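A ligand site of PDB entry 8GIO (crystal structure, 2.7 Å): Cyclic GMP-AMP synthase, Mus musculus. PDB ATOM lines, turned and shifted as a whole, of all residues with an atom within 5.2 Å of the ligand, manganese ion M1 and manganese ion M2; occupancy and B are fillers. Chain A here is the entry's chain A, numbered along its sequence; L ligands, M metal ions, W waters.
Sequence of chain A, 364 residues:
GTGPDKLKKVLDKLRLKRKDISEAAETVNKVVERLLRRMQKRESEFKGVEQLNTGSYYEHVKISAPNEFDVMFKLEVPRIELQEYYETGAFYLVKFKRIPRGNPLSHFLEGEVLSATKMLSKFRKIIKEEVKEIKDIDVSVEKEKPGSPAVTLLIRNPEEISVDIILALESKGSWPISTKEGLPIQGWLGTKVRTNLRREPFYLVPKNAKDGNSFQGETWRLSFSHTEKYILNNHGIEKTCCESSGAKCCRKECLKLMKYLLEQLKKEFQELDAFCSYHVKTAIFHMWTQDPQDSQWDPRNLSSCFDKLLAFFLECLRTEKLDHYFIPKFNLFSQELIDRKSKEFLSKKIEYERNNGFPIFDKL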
ATOM      1  N   GLY A  55      -5.514  24.187 -11.330  1.00  0.00           N
ATOM      2  CA  GLY A  55      -5.224  24.208 -12.748  1.00  0.00           C
ATOM      3  C   GLY A  55      -4.056  23.317 -13.151  1.00  0.00           C
ATOM      4  O   GLY A  55      -3.527  22.533 -12.356  1.00  0.00           O
ATOM      5  N   SER A  56      -3.654  23.448 -14.417  1.00  0.00           N
ATOM      6  CA  SER A  56      -2.865  22.384 -15.045  1.00  0.00           C
ATOM      7  C   SER A  56      -1.490  22.273 -14.419  1.00  0.00           C
ATOM      8  O   SER A  56      -0.969  21.151 -14.256  1.00  0.00           O
ATOM      9  CB  SER A  56      -2.745  22.600 -16.554  1.00  0.00           C
ATOM     10  OG  SER A  56      -2.212  23.888 -16.845  1.00  0.00           O
ATOM     11  N   TYR A  57      -0.868  23.407 -14.057  1.00  0.00           N
ATOM     12  CA  TYR A  57       0.508  23.361 -13.567  1.00  0.00           C
ATOM     13  C   TYR A  57       0.619  22.528 -12.287  1.00  0.00           C
ATOM     14  O   TYR A  57       1.593  21.808 -12.084  1.00  0.00           O
ATOM     15  CB  TYR A  57       1.049  24.769 -13.356  1.00  0.00           C
ATOM     16  CG  TYR A  57       2.394  24.777 -12.668  1.00  0.00           C
ATOM     17  CD1 TYR A  57       3.581  24.614 -13.391  1.00  0.00           C
ATOM     18  CD2 TYR A  57       2.491  24.926 -11.299  1.00  0.00           C
ATOM     19  CE1 TYR A  57       4.811  24.617 -12.763  1.00  0.00           C
ATOM     20  CE2 TYR A  57       3.709  24.926 -10.652  1.00  0.00           C
ATOM     21  CZ  TYR A  57       4.867  24.754 -11.394  1.00  0.00           C
ATOM     22  OH  TYR A  57       6.065  24.761 -10.726  1.00  0.00           O
ATOM     23  N   GLU A  59      -1.723  20.170 -11.368  1.00  0.00           N
ATOM     24  CA  GLU A  59      -2.087  18.799 -11.678  1.00  0.00           C
ATOM     25  C   GLU A  59      -0.997  18.082 -12.482  1.00  0.00           C
ATOM     26  O   GLU A  59      -1.113  16.873 -12.696  1.00  0.00           O
ATOM     27  CB  GLU A  59      -3.417  18.757 -12.447  1.00  0.00           C
ATOM     28  CG  GLU A  59      -4.586  19.454 -11.714  1.00  0.00           C
ATOM     29  CD  GLU A  59      -5.692  19.968 -12.642  1.00  0.00           C
ATOM     30  OE1 GLU A  59      -5.435  20.150 -13.865  1.00  0.00           O
ATOM     31  OE2 GLU A  59      -6.834  20.187 -12.168  1.00  0.00           O
ATOM     32  N   LYS A  62       0.297  20.742 -17.344  1.00  0.00           N
ATOM     33  CA  LYS A  62       0.717  21.914 -18.115  1.00  0.00           C
ATOM     34  C   LYS A  62       1.714  21.504 -19.183  1.00  0.00           C
ATOM     35  O   LYS A  62       2.683  20.798 -18.890  1.00  0.00           O
ATOM     36  CB  LYS A  62       1.358  22.939 -17.186  1.00  0.00           C
ATOM     37  CG  LYS A  62       1.726  24.223 -17.857  1.00  0.00           C
ATOM     38  CD  LYS A  62       0.490  24.944 -18.296  1.00  0.00           C
ATOM     39  CE  LYS A  62       0.816  26.310 -18.867  1.00  0.00           C
ATOM     40  NZ  LYS A  62       1.154  26.281 -20.301  1.00  0.00           N
ATOM     41  N   GLU A  68       1.658  29.633 -17.480  1.00  0.00           N
ATOM     42  CA  GLU A  68       0.299  29.998 -17.072  1.00  0.00           C
ATOM     43  C   GLU A  68      -0.088  29.256 -15.804  1.00  0.00           C
ATOM     44  O   GLU A  68      -0.286  28.046 -15.837  1.00  0.00           O
ATOM     45  CB  GLU A  68      -0.698  29.729 -18.180  1.00  0.00           C
ATOM     46  CG  GLU A  68      -1.886  30.638 -18.117  1.00  0.00           C
ATOM     47  CD  GLU A  68      -3.025  30.066 -17.280  1.00  0.00           C
ATOM     48  OE1 GLU A  68      -2.999  28.883 -16.956  1.00  0.00           O
ATOM     49  OE2 GLU A  68      -3.965  30.811 -16.946  1.00  0.00           O
ATOM     50  N   PHE A  69      -0.226  30.000 -14.698  1.00  0.00           N
ATOM     51  CA  PHE A  69      -0.527  29.467 -13.377  1.00  0.00           C
ATOM     52  C   PHE A  69      -1.880  29.973 -12.934  1.00  0.00           C
ATOM     53  O   PHE A  69      -2.255  31.115 -13.222  1.00  0.00           O
ATOM     54  CB  PHE A  69       0.538  29.908 -12.329  1.00  0.00           C
ATOM     55  CG  PHE A  69       1.938  29.502 -12.688  1.00  0.00           C
ATOM     56  CD1 PHE A  69       2.617  30.125 -13.734  1.00  0.00           C
ATOM     57  CD2 PHE A  69       2.574  28.485 -11.988  1.00  0.00           C
ATOM     58  CE1 PHE A  69       3.880  29.751 -14.059  1.00  0.00           C
ATOM     59  CE2 PHE A  69       3.838  28.104 -12.319  1.00  0.00           C
ATOM     60  CZ  PHE A  69       4.488  28.730 -13.355  1.00  0.00           C
ATOM     61  N   ASP A  70      -2.628  29.128 -12.214  1.00  0.00           N
ATOM     62  CA  ASP A  70      -3.910  29.549 -11.654  1.00  0.00           C
ATOM     63  C   ASP A  70      -3.891  29.360 -10.156  1.00  0.00           C
ATOM     64  O   ASP A  70      -3.474  28.309  -9.668  1.00  0.00           O
ATOM     65  CB  ASP A  70      -5.087  28.765 -12.237  1.00  0.00           C
ATOM     66  CG  ASP A  70      -4.994  28.594 -13.713  1.00  0.00           C
ATOM     67  OD1 ASP A  70      -5.246  29.583 -14.431  1.00  0.00           O
ATOM     68  OD2 ASP A  70      -4.630  27.492 -14.158  1.00  0.00           O
ATOM     69  N   ASP A 164      -3.575  33.754 -13.155  1.00  0.00           N
ATOM     70  CA  ASP A 164      -4.955  34.107 -12.856  1.00  0.00           C
ATOM     71  C   ASP A 164      -5.190  34.045 -11.345  1.00  0.00           C
ATOM     72  O   ASP A 164      -5.244  32.950 -10.773  1.00  0.00           O
ATOM     73  CB  ASP A 164      -5.902  33.156 -13.575  1.00  0.00           C
ATOM     74  CG  ASP A 164      -5.857  33.319 -15.055  1.00  0.00           C
ATOM     75  OD1 ASP A 164      -5.700  34.468 -15.503  1.00  0.00           O
ATOM     76  OD2 ASP A 164      -5.972  32.324 -15.789  1.00  0.00           O
ATOM     77  N   ARG A 221     -20.697  31.561 -10.025  1.00  0.00           N
ATOM     78  CA  ARG A 221     -20.596  30.253 -10.667  1.00  0.00           C
ATOM     79  C   ARG A 221     -19.887  29.276  -9.751  1.00  0.00           C
ATOM     80  O   ARG A 221     -18.892  29.628  -9.104  1.00  0.00           O
ATOM     81  CB  ARG A 221     -19.832  30.352 -12.006  1.00  0.00           C
ATOM     82  CG  ARG A 221     -19.756  29.035 -12.792  1.00  0.00           C
ATOM     83  CD  ARG A 221     -18.563  28.969 -13.746  1.00  0.00           C
ATOM     84  NE  ARG A 221     -17.374  28.407 -13.110  1.00  0.00           N
ATOM     85  CZ  ARG A 221     -16.147  28.863 -13.308  1.00  0.00           C
ATOM     86  NH1 ARG A 221     -15.906  29.852 -14.163  1.00  0.00           N
ATOM     87  NH2 ARG A 221     -15.123  28.330 -12.634  1.00  0.00           N
ATOM     88  N   LEU A 222     -20.386  28.034  -9.695  1.00  0.00           N
ATOM     89  CA  LEU A 222     -19.733  27.007  -8.876  1.00  0.00           C
ATOM     90  C   LEU A 222     -18.357  26.671  -9.454  1.00  0.00           C
ATOM     91  O   LEU A 222     -18.146  26.726 -10.669  1.00  0.00           O
ATOM     92  CB  LEU A 222     -20.598  25.748  -8.826  1.00  0.00           C
ATOM     93  CG  LEU A 222     -21.776  25.731  -7.852  1.00  0.00           C
ATOM     94  CD1 LEU A 222     -22.763  24.630  -8.110  1.00  0.00           C
ATOM     95  CD2 LEU A 222     -21.230  25.610  -6.431  1.00  0.00           C
ATOM     96  N   PHE A 224     -15.029  23.756  -8.974  1.00  0.00           N
ATOM     97  CA  PHE A 224     -14.542  22.535  -8.364  1.00  0.00           C
ATOM     98  C   PHE A 224     -13.075  22.299  -8.688  1.00  0.00           C
ATOM     99  O   PHE A 224     -12.622  21.158  -8.734  1.00  0.00           O
ATOM    100  CB  PHE A 224     -15.403  21.342  -8.801  1.00  0.00           C
ATOM    101  CG  PHE A 224     -16.816  21.436  -8.327  1.00  0.00           C
ATOM    102  CD1 PHE A 224     -17.155  21.094  -7.031  1.00  0.00           C
ATOM    103  CD2 PHE A 224     -17.814  21.887  -9.165  1.00  0.00           C
ATOM    104  CE1 PHE A 224     -18.431  21.171  -6.578  1.00  0.00           C
ATOM    105  CE2 PHE A 224     -19.123  21.978  -8.730  1.00  0.00           C
ATOM    106  CZ  PHE A 224     -19.438  21.626  -7.421  1.00  0.00           C
ATOM    107  N   SER A 225     -12.304  23.366  -8.946  1.00  0.00           N
ATOM    108  CA  SER A 225     -10.901  23.180  -9.269  1.00  0.00           C
ATOM    109  C   SER A 225     -10.234  22.331  -8.213  1.00  0.00           C
ATOM    110  O   SER A 225      -9.324  21.567  -8.526  1.00  0.00           O
ATOM    111  CB  SER A 225     -10.152  24.504  -9.366  1.00  0.00           C
ATOM    112  OG  SER A 225     -10.596  25.276 -10.450  1.00  0.00           O
ATOM    113  N   GLU A 228     -11.027  18.689  -8.821  1.00  0.00           N
ATOM    114  CA  GLU A 228     -10.347  18.245 -10.027  1.00  0.00           C
ATOM    115  C   GLU A 228      -8.845  18.071  -9.812  1.00  0.00           C
ATOM    116  O   GLU A 228      -8.231  17.169 -10.387  1.00  0.00           O
ATOM    117  CB  GLU A 228     -10.645  19.227 -11.149  1.00  0.00           C
ATOM    118  CG  GLU A 228     -12.141  19.496 -11.320  1.00  0.00           C
ATOM    119  CD  GLU A 228     -12.389  20.666 -12.245  1.00  0.00           C
ATOM    120  OE1 GLU A 228     -11.398  21.176 -12.802  1.00  0.00           O
ATOM    121  OE2 GLU A 228     -13.559  21.069 -12.424  1.00  0.00           O
ATOM    122  N   LYS A 259      -5.041  18.327 -24.953  1.00  0.00           N
ATOM    123  CA  LYS A 259      -4.846  19.745 -24.673  1.00  0.00           C
ATOM    124  C   LYS A 259      -4.092  20.401 -25.815  1.00  0.00           C
ATOM    125  O   LYS A 259      -4.457  21.476 -26.316  1.00  0.00           O
ATOM    126  CB  LYS A 259      -4.085  19.937 -23.362  1.00  0.00           C
ATOM    127  CG  LYS A 259      -4.916  19.715 -22.112  1.00  0.00           C
ATOM    128  CD  LYS A 259      -4.011  19.567 -20.893  1.00  0.00           C
ATOM    129  CE  LYS A 259      -3.183  20.834 -20.679  1.00  0.00           C
ATOM    130  NZ  LYS A 259      -4.022  21.978 -20.236  1.00  0.00           N
ATOM    131  N   GLU A 263      -4.871  23.411 -28.308  1.00  0.00           N
ATOM    132  CA  GLU A 263      -4.071  24.632 -28.240  1.00  0.00           C
ATOM    133  C   GLU A 263      -3.557  25.026 -29.622  1.00  0.00           C
ATOM    134  O   GLU A 263      -3.611  26.200 -30.013  1.00  0.00           O
ATOM    135  CB  GLU A 263      -2.892  24.447 -27.276  1.00  0.00           C
ATOM    136  CG  GLU A 263      -3.205  24.757 -25.843  1.00  0.00           C
ATOM    137  CD  GLU A 263      -1.975  24.767 -24.933  1.00  0.00           C
ATOM    138  OE1 GLU A 263      -0.869  25.068 -25.444  1.00  0.00           O
ATOM    139  OE2 GLU A 263      -2.105  24.464 -23.705  1.00  0.00           O
ATOM    140  N   CYS A 276     -12.278  25.903 -25.056  1.00  0.00           N
ATOM    141  CA  CYS A 276     -11.294  26.140 -24.020  1.00  0.00           C
ATOM    142  C   CYS A 276     -10.823  24.791 -23.507  1.00  0.00           C
ATOM    143  O   CYS A 276     -11.402  23.761 -23.819  1.00  0.00           O
ATOM    144  CB  CYS A 276     -11.845  27.023 -22.887  1.00  0.00           C
ATOM    145  SG  CYS A 276     -13.041  26.245 -21.785  1.00  0.00           S
ATOM    146  N   SER A 277      -9.766  24.807 -22.700  1.00  0.00           N
ATOM    147  CA  SER A 277      -9.188  23.533 -22.331  1.00  0.00           C
ATOM    148  C   SER A 277     -10.089  22.782 -21.358  1.00  0.00           C
ATOM    149  O   SER A 277      -9.952  21.558 -21.212  1.00  0.00           O
ATOM    150  CB  SER A 277      -7.779  23.724 -21.777  1.00  0.00           C
ATOM    151  OG  SER A 277      -7.794  24.383 -20.538  1.00  0.00           O
ATOM    152  N   TYR A 278     -11.031  23.480 -20.711  1.00  0.00           N
ATOM    153  CA  TYR A 278     -11.894  22.806 -19.749  1.00  0.00           C
ATOM    154  C   TYR A 278     -12.836  21.837 -20.447  1.00  0.00           C
ATOM    155  O   TYR A 278     -13.224  20.802 -19.879  1.00  0.00           O
ATOM    156  CB  TYR A 278     -12.682  23.842 -18.936  1.00  0.00           C
ATOM    157  CG  TYR A 278     -13.389  23.256 -17.737  1.00  0.00           C
ATOM    158  CD1 TYR A 278     -12.672  22.807 -16.634  1.00  0.00           C
ATOM    159  CD2 TYR A 278     -14.795  23.146 -17.698  1.00  0.00           C
ATOM    160  CE1 TYR A 278     -13.300  22.268 -15.501  1.00  0.00           C
ATOM    161  CE2 TYR A 278     -15.445  22.594 -16.580  1.00  0.00           C
ATOM    162  CZ  TYR A 278     -14.681  22.163 -15.483  1.00  0.00           C
ATOM    163  OH  TYR A 278     -15.273  21.624 -14.348  1.00  0.00           O
ATOM    164  N   LYS A 281     -10.767  18.816 -20.599  1.00  0.00           N
ATOM    165  CA  LYS A 281     -10.681  18.192 -19.285  1.00  0.00           C
ATOM    166  C   LYS A 281     -11.966  17.479 -18.932  1.00  0.00           C
ATOM    167  O   LYS A 281     -11.950  16.356 -18.402  1.00  0.00           O
ATOM    168  CB  LYS A 281     -10.362  19.262 -18.235  1.00  0.00           C
ATOM    169  CG  LYS A 281      -9.860  18.794 -16.874  1.00  0.00           C
ATOM    170  CD  LYS A 281      -9.662  20.017 -15.974  1.00  0.00           C
ATOM    171  CE  LYS A 281      -8.847  19.690 -14.705  1.00  0.00           C
ATOM    172  NZ  LYS A 281      -8.774  20.841 -13.740  1.00  0.00           N
ATOM    173  N   HIS A 324     -21.305  19.066 -17.944  1.00  0.00           N
ATOM    174  CA  HIS A 324     -20.448  19.368 -16.818  1.00  0.00           C
ATOM    175  C   HIS A 324     -20.326  18.145 -15.926  1.00  0.00           C
ATOM    176  O   HIS A 324     -21.323  17.490 -15.616  1.00  0.00           O
ATOM    177  CB  HIS A 324     -21.052  20.543 -16.038  1.00  0.00           C
ATOM    178  CG  HIS A 324     -20.091  21.230 -15.122  1.00  0.00           C
ATOM    179  ND1 HIS A 324     -19.482  20.589 -14.063  1.00  0.00           N
ATOM    180  CD2 HIS A 324     -19.643  22.506 -15.097  1.00  0.00           C
ATOM    181  CE1 HIS A 324     -18.690  21.438 -13.429  1.00  0.00           C
ATOM    182  NE2 HIS A 324     -18.766  22.603 -14.040  1.00  0.00           N
HETATM  183  P1  LIG L   1      -4.360  25.172 -19.238  1.00  0.00           P
HETATM  184  O1  LIG L   1      -5.001  25.207 -20.594  1.00  0.00           O
HETATM  185  O2  LIG L   1      -2.973  24.501 -19.233  1.00  0.00           O
HETATM  186  O3  LIG L   1      -4.298  26.551 -18.597  1.00  0.00           O
HETATM  187  P2  LIG L   1      -6.253  24.533 -17.008  1.00  0.00           P
HETATM  188  O4  LIG L   1      -7.125  23.391 -16.666  1.00  0.00           O
HETATM  189  O5  LIG L   1      -5.425  25.069 -15.846  1.00  0.00           O
HETATM  190  O6  LIG L   1      -5.243  24.297 -18.214  1.00  0.00           O
HETATM  191  P3  LIG L   1      -7.443  27.223 -17.149  1.00  0.00           P
HETATM  192  O7  LIG L   1      -8.159  27.872 -18.251  1.00  0.00           O
HETATM  193  O8  LIG L   1      -6.098  27.756 -16.654  1.00  0.00           O
HETATM  194  O9  LIG L   1      -7.127  25.728 -17.569  1.00  0.00           O
HETATM  195  O10 LIG L   1      -8.468  27.106 -15.948  1.00  0.00           O
HETATM  196  C1  LIG L   1      -8.025  26.892 -14.591  1.00  0.00           C
HETATM  197  C2  LIG L   1      -8.989  25.982 -13.834  1.00  0.00           C
HETATM  198  O11 LIG L   1     -10.227  26.692 -13.606  1.00  0.00           O
HETATM  199  C3  LIG L   1      -9.401  24.687 -14.522  1.00  0.00           C
HETATM  200  O12 LIG L   1      -8.497  23.626 -14.234  1.00  0.00           O
HETATM  201  C4  LIG L   1     -10.778  24.411 -13.911  1.00  0.00           C
HETATM  202  O13 LIG L   1     -10.696  23.857 -12.601  1.00  0.00           O
HETATM  203  C5  LIG L   1     -11.341  25.824 -13.754  1.00  0.00           C
HETATM  204  N1  LIG L   1     -12.135  26.284 -14.885  1.00  0.00           N
HETATM  205  C6  LIG L   1     -11.672  26.936 -16.002  1.00  0.00           C
HETATM  206  N2  LIG L   1     -12.610  27.233 -16.874  1.00  0.00           N
HETATM  207  C7  LIG L   1     -13.773  26.755 -16.283  1.00  0.00           C
HETATM  208  C8  LIG L   1     -15.112  26.752 -16.702  1.00  0.00           C
HETATM  209  N3  LIG L   1     -15.537  27.282 -17.857  1.00  0.00           N
HETATM  210  N4  LIG L   1     -16.037  26.199 -15.865  1.00  0.00           N
HETATM  211  C9  LIG L   1     -15.617  25.648 -14.717  1.00  0.00           C
HETATM  212  N5  LIG L   1     -14.376  25.582 -14.237  1.00  0.00           N
HETATM  213  C10 LIG L   1     -13.495  26.161 -15.059  1.00  0.00           C
HETATM  214 MN    MN M   1      -3.745  26.727 -16.436  1.00  0.00          MN
HETATM  215 MN    MN M   2      -6.317  30.231 -16.564  1.00  0.00          MN
HETATM  216  O   HOH W   1      -1.053  23.906 -21.021  1.00  0.00           O
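A nitrogen (N5) of the ligand sits at hydrogen-bond distance from the guanidinium group of Arg 221 (3.3 Å). An oxygen (O5) of the ligand lies close to the backbone NH of Ser 56, 2.8 Å away. NZ of Lys 259 is in salt-bridge range of O2 of the ligand. The side-chain carboxylate (OE1) of Glu 228 lies within hydrogen-bond range of an oxygen (O13) of the ligand. The side-chain hydroxyl of Ser 56 sits at hydrogen-bond distance from an oxygen (O2) of the ligand. The side-chain hydroxyl of Ser 277 lies within hydrogen-bond range of an oxygen (O1) of the ligand (2.9 Å). The side-chain hydroxyl of Ser 225 sits at hydrogen-bond distance from an oxygen (O13) of the ligand (2.6 Å). O12 of the ligand lies within hydrogen-bond range of NZ of Lys 281 (2.8 Å).
OH of Tyr 278 is in hydrogen-bond range of OE2 of Glu 228, at 2.6 Å. The backbone NH of Lys 62 sits at hydrogen-bond distance from the backbone carbonyl oxygen of Ser 56 (3.4 Å). N of Tyr 278 sits close to SG of Cys 276 (3.6 Å). OE1 of Glu 228 is in salt-bridge range of NZ of Lys 281 (2.8 Å). The backbone carbonyl oxygen (O) of Phe 69 sits at hydrogen-bond distance from the backbone NH (N) of Asp 164, 3.0 Å away. The side-chain amino group of Lys 281 is in salt-bridge range of the side-chain carboxylate of Glu 59 (2.6 Å).
Residues that only touch the ligand: Gly 55 (3.2 Å), Lys 62 (3.6 Å) and Tyr 278 (3.6 Å).
Ser 56 touches manganese ion M1 (OG to MN, 3.3 Å). Three residues have an atom within 4 Å of manganese ion M1: Ser 56, Glu 68 and Asp 70. The nearest printed residue that does not touch manganese ion M1 is Gly 55 (4.7 Å).
Of the 21 residues printed, 3 come within 4 Å of manganese ion M2. The nearest printed residue that does not touch manganese ion M2 is Phe 69 (5.3 Å).
Manganese ion M1 is bound by O3 of the ligand (2.2 Å), OE1 of Glu 68 (2.3 Å), O5 of the ligand (2.4 Å), OD2 of Asp 70 (2.6 Å) and O8 of the ligand (2.6 Å). Manganese ion M1 has five donor atoms within binding distance.
Manganese ion M2 is bound by OD2 of Asp 164 (2.3 Å), OE2 of Glu 68 (2.5 Å), OD1 of Asp 70 (2.5 Å) and O8 of the ligand (2.5 Å). Manganese ion M2 has four donor atoms within binding distance.
Water W1 lies within hydrogen-bond range of O2 of the ligand, OE2 of Glu 263 and NZ of Lys 62.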
